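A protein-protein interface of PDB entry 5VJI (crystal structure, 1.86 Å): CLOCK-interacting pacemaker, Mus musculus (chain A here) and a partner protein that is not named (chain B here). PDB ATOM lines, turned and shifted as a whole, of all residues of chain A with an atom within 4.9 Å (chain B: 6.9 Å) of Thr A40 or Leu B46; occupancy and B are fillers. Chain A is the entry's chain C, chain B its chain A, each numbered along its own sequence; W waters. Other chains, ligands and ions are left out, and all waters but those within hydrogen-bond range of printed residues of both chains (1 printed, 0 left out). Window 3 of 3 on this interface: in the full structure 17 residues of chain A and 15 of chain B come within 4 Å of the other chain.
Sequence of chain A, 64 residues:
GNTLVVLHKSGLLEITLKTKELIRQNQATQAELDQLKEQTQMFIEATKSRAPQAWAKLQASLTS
Among the printed residues, merely in contact across the chains: Lys A37 with Ile B42 (3.9 Å), Thr A40 with Ile B42 (3.5 Å), Thr A40 with Leu B46 (3.98 Å), Phe A43 with Leu B46 (3.995 Å), Phe A43 with Val B49 (3.9 Å), Ile A44 with Gln B45 (3.9 Å) and Ile A44 with Val B49 (3.4 Å).
Of the printed residues of chain B, Thr A40 touches Ile B42 and Leu B46. Of the printed residues of chain A, Leu B46 touches Thr A40 (3.98 Å) and Phe A43 (3.995 Å). Of the printed residues of chain B, Ile A44 touches Gln B45 and Val B49. Of the printed residues of chain B, Phe A43 touches Leu B46 (3.995 Å) and Val B49 (3.9 Å). Of the printed residues of chain B, Lys A37 touches Ile B42. Glu A45 touches none of the printed residues of chain B. The nearest printed residue of chain A that does not touch Leu B46 is Ile A44 (4.4 Å). The nearest printed residue of chain B that does not touch Ile A44 is Leu B46 (4.4 Å).
Water W1 lies within hydrogen-bond range of OE1 of Gln B45 (3.0 Å), O of Lys A37 (3.1 Å) and NE2 of Gln A41 (3.4 Å).
Hydrophobic or aromatic side chains of chain B within 4 Å of the printed part of chain A: Ile B42, Leu B46 and Val B49. Of the 10 printed residues of chain A, 4 touch a printed residue of chain B. Hydrophobic or aromatic side chains of chain A within 4 Å of the printed part of chain B: Phe A43 and Ile A44. Among the printed residues, 7 pairs touch across the chains. Among the printed residues, no Asp or Glu carboxylate lies within 4 Å of a Lys or Arg side-chain nitrogen of the other chain.
The side-chain hydroxyl (OG1) of Thr A40 sits at hydrogen-bond distance from the backbone carbonyl oxygen (O) of Leu A36 (2.9 Å).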
ATOM      1  N   LEU A  36     -13.378  21.307  26.165  1.00  0.00           N
ATOM      2  CA  LEU A  36     -12.903  19.978  26.605  1.00  0.00           C
ATOM      3  C   LEU A  36     -11.587  19.602  25.932  1.00  0.00           C
ATOM      4  O   LEU A  36     -10.695  19.032  26.579  1.00  0.00           O
ATOM      5  CB  LEU A  36     -13.979  18.931  26.306  1.00  0.00           C
ATOM      6  CG  LEU A  36     -13.627  17.521  26.757  1.00  0.00           C
ATOM      7  CD1 LEU A  36     -13.366  17.540  28.250  1.00  0.00           C
ATOM      8  CD2 LEU A  36     -14.791  16.554  26.368  1.00  0.00           C
ATOM      9  N   LYS A  37     -11.453  19.925  24.634  1.00  0.00           N
ATOM     10  CA  LYS A  37     -10.204  19.759  23.904  1.00  0.00           C
ATOM     11  C   LYS A  37      -9.059  20.435  24.635  1.00  0.00           C
ATOM     12  O   LYS A  37      -7.966  19.853  24.776  1.00  0.00           O
ATOM     13  CB  LYS A  37     -10.319  20.365  22.485  1.00  0.00           C
ATOM     14  CG  LYS A  37     -10.957  19.526  21.420  1.00  0.00           C
ATOM     15  CD  LYS A  37     -10.889  20.288  20.077  1.00  0.00           C
ATOM     16  CE  LYS A  37     -11.855  19.738  19.014  1.00  0.00           C
ATOM     17  NZ  LYS A  37     -12.362  20.848  18.097  1.00  0.00           N
ATOM     18  N   GLU A  38      -9.270  21.697  25.062  1.00  0.00           N
ATOM     19  CA  GLU A  38      -8.181  22.460  25.693  1.00  0.00           C
ATOM     20  C   GLU A  38      -7.812  21.858  27.048  1.00  0.00           C
ATOM     21  O   GLU A  38      -6.632  21.703  27.363  1.00  0.00           O
ATOM     22  CB  GLU A  38      -8.563  23.938  25.887  1.00  0.00           C
ATOM     23  CG  GLU A  38      -9.278  24.582  24.702  1.00  0.00           C
ATOM     24  CD  GLU A  38      -9.810  25.985  25.001  1.00  0.00           C
ATOM     25  OE1 GLU A  38      -9.591  26.474  26.139  1.00  0.00           O
ATOM     26  OE2 GLU A  38     -10.432  26.598  24.089  1.00  0.00           O
ATOM     27  N   GLN A  39      -8.820  21.505  27.853  1.00  0.00           N
ATOM     28  CA  GLN A  39      -8.591  20.868  29.150  1.00  0.00           C
ATOM     29  C   GLN A  39      -7.881  19.529  29.020  1.00  0.00           C
ATOM     30  O   GLN A  39      -6.988  19.218  29.817  1.00  0.00           O
ATOM     31  CB  GLN A  39      -9.928  20.661  29.886  1.00  0.00           C
ATOM     32  CG  GLN A  39     -10.556  21.925  30.381  1.00  0.00           C
ATOM     33  CD  GLN A  39     -12.053  21.773  30.543  1.00  0.00           C
ATOM     34  OE1 GLN A  39     -12.638  20.768  30.105  1.00  0.00           O
ATOM     35  NE2 GLN A  39     -12.692  22.759  31.161  1.00  0.00           N
ATOM     36  N   THR A  40      -8.293  18.703  28.059  1.00  0.00           N
ATOM     37  CA  THR A  40      -7.598  17.437  27.788  1.00  0.00           C
ATOM     38  C   THR A  40      -6.141  17.672  27.399  1.00  0.00           C
ATOM     39  O   THR A  40      -5.219  17.077  27.974  1.00  0.00           O
ATOM     40  CB  THR A  40      -8.378  16.681  26.706  1.00  0.00           C
ATOM     41  OG1 THR A  40      -9.694  16.376  27.238  1.00  0.00           O
ATOM     42  CG2 THR A  40      -7.682  15.381  26.324  1.00  0.00           C
ATOM     43  N   GLN A  41      -5.908  18.588  26.465  1.00  0.00           N
ATOM     44  CA  GLN A  41      -4.544  18.864  26.035  1.00  0.00           C
ATOM     45  C   GLN A  41      -3.697  19.370  27.202  1.00  0.00           C
ATOM     46  O   GLN A  41      -2.512  19.037  27.312  1.00  0.00           O
ATOM     47  CB  GLN A  41      -4.541  19.869  24.878  1.00  0.00           C
ATOM     48  CG  GLN A  41      -4.549  19.237  23.480  1.00  0.00           C
ATOM     49  CD  GLN A  41      -4.743  20.278  22.360  1.00  0.00           C
ATOM     50  OE1 GLN A  41      -4.058  21.311  22.334  1.00  0.00           O
ATOM     51  NE2 GLN A  41      -5.681  20.007  21.434  1.00  0.00           N
ATOM     52  N   MET A  42      -4.282  20.169  28.075  1.00  0.00           N
ATOM     53  CA  MET A  42      -3.558  20.682  29.232  1.00  0.00           C
ATOM     54  C   MET A  42      -3.193  19.538  30.178  1.00  0.00           C
ATOM     55  O   MET A  42      -2.085  19.492  30.731  1.00  0.00           O
ATOM     56  CB  MET A  42      -4.396  21.724  29.954  1.00  0.00           C
ATOM     57  CG  MET A  42      -3.813  22.205  31.264  1.00  0.00           C
ATOM     58  SD  MET A  42      -4.884  23.660  32.003  1.00  0.00           S
ATOM     59  CE  MET A  42      -4.773  24.928  30.511  1.00  0.00           C
ATOM     60  N   PHE A  43      -4.151  18.632  30.375  1.00  0.00           N
ATOM     61  CA  PHE A  43      -3.958  17.478  31.251  1.00  0.00           C
ATOM     62  C   PHE A  43      -2.890  16.553  30.698  1.00  0.00           C
ATOM     63  O   PHE A  43      -1.973  16.137  31.418  1.00  0.00           O
ATOM     64  CB  PHE A  43      -5.311  16.737  31.422  1.00  0.00           C
ATOM     65  CG  PHE A  43      -5.199  15.407  32.141  1.00  0.00           C
ATOM     66  CD1 PHE A  43      -4.640  15.334  33.400  1.00  0.00           C
ATOM     67  CD2 PHE A  43      -5.625  14.246  31.541  1.00  0.00           C
ATOM     68  CE1 PHE A  43      -4.485  14.098  34.081  1.00  0.00           C
ATOM     69  CE2 PHE A  43      -5.521  13.012  32.199  1.00  0.00           C
ATOM     70  CZ  PHE A  43      -4.961  12.937  33.479  1.00  0.00           C
ATOM     71  N   ILE A  44      -2.948  16.257  29.401  1.00  0.00           N
ATOM     72  CA  ILE A  44      -1.925  15.401  28.802  1.00  0.00           C
ATOM     73  C   ILE A  44      -0.549  16.050  28.906  1.00  0.00           C
ATOM     74  O   ILE A  44       0.427  15.388  29.257  1.00  0.00           O
ATOM     75  CB  ILE A  44      -2.264  15.084  27.332  1.00  0.00           C
ATOM     76  CG1 ILE A  44      -3.618  14.391  27.187  1.00  0.00           C
ATOM     77  CG2 ILE A  44      -1.097  14.301  26.659  1.00  0.00           C
ATOM     78  CD1 ILE A  44      -3.893  13.315  28.153  1.00  0.00           C
ATOM     79  N   GLU A  45      -0.443  17.351  28.574  1.00  0.00           N
ATOM     80  CA  GLU A  45       0.825  18.069  28.706  1.00  0.00           C
ATOM     81  C   GLU A  45       1.394  17.970  30.117  1.00  0.00           C
ATOM     82  O   GLU A  45       2.606  17.750  30.305  1.00  0.00           O
ATOM     83  CB  GLU A  45       0.636  19.535  28.346  1.00  0.00           C
ATOM     84  CG  GLU A  45       0.827  19.850  26.874  1.00  0.00           C
ATOM     85  CD  GLU A  45      -0.125  20.913  26.358  1.00  0.00           C
ATOM     86  OE1 GLU A  45      -0.457  21.851  27.115  1.00  0.00           O
ATOM     87  OE2 GLU A  45      -0.542  20.808  25.188  1.00  0.00           O
ATOM     88  N   LYS B  41     -11.192  11.451  19.122  1.00  0.00           N
ATOM     89  CA  LYS B  41      -9.797  11.837  19.315  1.00  0.00           C
ATOM     90  C   LYS B  41      -9.478  12.122  20.786  1.00  0.00           C
ATOM     91  O   LYS B  41      -8.408  11.761  21.271  1.00  0.00           O
ATOM     92  CB  LYS B  41      -9.463  13.083  18.483  1.00  0.00           C
ATOM     93  CG  LYS B  41      -9.120  12.818  17.024  1.00  0.00           C
ATOM     94  CD  LYS B  41      -8.282  13.958  16.443  1.00  0.00           C
ATOM     95  CE  LYS B  41      -9.096  14.885  15.564  1.00  0.00           C
ATOM     96  NZ  LYS B  41      -9.479  14.206  14.288  1.00  0.00           N
ATOM     97  N   ILE B  42     -10.362  12.837  21.483  1.00  0.00           N
ATOM     98  CA  ILE B  42     -10.154  13.130  22.894  1.00  0.00           C
ATOM     99  C   ILE B  42     -10.126  11.839  23.708  1.00  0.00           C
ATOM    100  O   ILE B  42      -9.308  11.690  24.615  1.00  0.00           O
ATOM    101  CB  ILE B  42     -11.250  14.081  23.415  1.00  0.00           C
ATOM    102  CG1 ILE B  42     -11.132  15.466  22.780  1.00  0.00           C
ATOM    103  CG2 ILE B  42     -11.239  14.120  24.974  1.00  0.00           C
ATOM    104  CD1 ILE B  42     -12.418  16.303  22.974  1.00  0.00           C
ATOM    105  N   GLN B  43     -11.047  10.902  23.412  1.00  0.00           N
ATOM    106  CA  GLN B  43     -11.078   9.638  24.145  1.00  0.00           C
ATOM    107  C   GLN B  43      -9.775   8.864  23.916  1.00  0.00           C
ATOM    108  O   GLN B  43      -9.185   8.320  24.854  1.00  0.00           O
ATOM    109  CB  GLN B  43     -12.323   8.825  23.715  1.00  0.00           C
ATOM    110  CG  GLN B  43     -13.607   9.401  24.308  1.00  0.00           C
ATOM    111  CD  GLN B  43     -14.873   8.676  23.869  1.00  0.00           C
ATOM    112  OE1 GLN B  43     -14.863   7.921  22.894  1.00  0.00           O
ATOM    113  NE2 GLN B  43     -15.975   8.931  24.577  1.00  0.00           N
ATOM    114  N   GLU B  44      -9.268   8.879  22.680  1.00  0.00           N
ATOM    115  CA  GLU B  44      -8.040   8.155  22.342  1.00  0.00           C
ATOM    116  C   GLU B  44      -6.836   8.716  23.101  1.00  0.00           C
ATOM    117  O   GLU B  44      -5.991   7.956  23.596  1.00  0.00           O
ATOM    118  CB  GLU B  44      -7.808   8.260  20.829  1.00  0.00           C
ATOM    119  CG  GLU B  44      -7.330   7.016  20.087  1.00  0.00           C
ATOM    120  CD  GLU B  44      -7.580   7.132  18.559  1.00  0.00           C
ATOM    121  OE1 GLU B  44      -7.303   8.210  17.981  1.00  0.00           O
ATOM    122  OE2 GLU B  44      -8.082   6.158  17.947  1.00  0.00           O
ATOM    123  N   GLN B  45      -6.744  10.042  23.188  1.00  0.00           N
ATOM    124  CA  GLN B  45      -5.680  10.717  23.943  1.00  0.00           C
ATOM    125  C   GLN B  45      -5.732  10.377  25.435  1.00  0.00           C
ATOM    126  O   GLN B  45      -4.688  10.153  26.069  1.00  0.00           O
ATOM    127  CB  GLN B  45      -5.794  12.241  23.736  1.00  0.00           C
ATOM    128  CG  GLN B  45      -5.472  12.682  22.337  1.00  0.00           C
ATOM    129  CD  GLN B  45      -4.898  14.090  22.267  1.00  0.00           C
ATOM    130  OE1 GLN B  45      -5.422  15.034  22.872  1.00  0.00           O
ATOM    131  NE2 GLN B  45      -3.799  14.234  21.527  1.00  0.00           N
ATOM    132  N   LEU B  46      -6.943  10.354  26.018  1.00  0.00           N
ATOM    133  CA  LEU B  46      -7.069  10.052  27.449  1.00  0.00           C
ATOM    134  C   LEU B  46      -6.645   8.625  27.750  1.00  0.00           C
ATOM    135  O   LEU B  46      -6.061   8.351  28.810  1.00  0.00           O
ATOM    136  CB  LEU B  46      -8.507  10.264  27.930  1.00  0.00           C
ATOM    137  CG  LEU B  46      -8.962  11.720  27.965  1.00  0.00           C
ATOM    138  CD1 LEU B  46     -10.449  11.821  28.246  1.00  0.00           C
ATOM    139  CD2 LEU B  46      -8.149  12.473  29.002  1.00  0.00           C
ATOM    140  N   GLN B  47      -6.941   7.699  26.851  1.00  0.00           N
ATOM    141  CA  GLN B  47      -6.544   6.327  27.156  1.00  0.00           C
ATOM    142  C   GLN B  47      -5.036   6.119  27.123  1.00  0.00           C
ATOM    143  O   GLN B  47      -4.563   5.067  27.565  1.00  0.00           O
ATOM    144  CB  GLN B  47      -7.223   5.340  26.205  1.00  0.00           C
ATOM    145  CG  GLN B  47      -8.753   5.366  26.222  1.00  0.00           C
ATOM    146  CD  GLN B  47      -9.389   4.959  27.554  1.00  0.00           C
ATOM    147  OE1 GLN B  47     -10.537   5.310  27.832  1.00  0.00           O
ATOM    148  NE2 GLN B  47      -8.661   4.202  28.363  1.00  0.00           N
ATOM    149  N   MET B  48      -4.261   7.078  26.634  1.00  0.00           N
ATOM    150  CA  MET B  48      -2.799   6.963  26.595  1.00  0.00           C
ATOM    151  C   MET B  48      -2.179   7.236  27.970  1.00  0.00           C
ATOM    152  O   MET B  48      -1.037   6.859  28.229  1.00  0.00           O
ATOM    153  CB  MET B  48      -2.193   7.922  25.552  1.00  0.00           C
ATOM    154  CG  MET B  48      -2.406   7.519  24.084  1.00  0.00           C
ATOM    155  SD  MET B  48      -1.581   8.724  22.750  1.00  0.00           S
ATOM    156  CE  MET B  48      -2.458   8.060  21.135  1.00  0.00           C
ATOM    157  N   VAL B  49      -2.937   7.911  28.849  1.00  0.00           N
ATOM    158  CA  VAL B  49      -2.493   8.209  30.215  1.00  0.00           C
ATOM    159  C   VAL B  49      -2.507   6.938  31.061  1.00  0.00           C
ATOM    160  O   VAL B  49      -3.346   6.044  30.872  1.00  0.00           O
ATOM    161  CB  VAL B  49      -3.392   9.290  30.850  1.00  0.00           C
ATOM    162  CG1 VAL B  49      -2.879   9.682  32.202  1.00  0.00           C
ATOM    163  CG2 VAL B  49      -3.466  10.505  29.953  1.00  0.00           C
ATOM    164  N   HIS B  50      -1.586   6.865  32.023  1.00  0.00           N
ATOM    165  CA  HIS B  50      -1.595   5.791  33.017  1.00  0.00           C
ATOM    166  C   HIS B  50      -2.283   6.243  34.306  1.00  0.00           C
ATOM    167  O   HIS B  50      -3.124   7.150  34.304  1.00  0.00           O
ATOM    168  CB  HIS B  50      -0.173   5.321  33.328  1.00  0.00           C
ATOM    169  CG  HIS B  50       0.602   4.894  32.121  1.00  0.00           C
ATOM    170  ND1 HIS B  50       0.098   4.981  30.841  1.00  0.00           N
ATOM    171  CD2 HIS B  50       1.848   4.379  31.999  1.00  0.00           C
ATOM    172  CE1 HIS B  50       1.001   4.543  29.982  1.00  0.00           C
ATOM    173  NE2 HIS B  50       2.072   4.170  30.659  1.00  0.00           N
HETATM  174  O   HOH W   1      -7.232  17.439  22.928  1.00  0.00           O
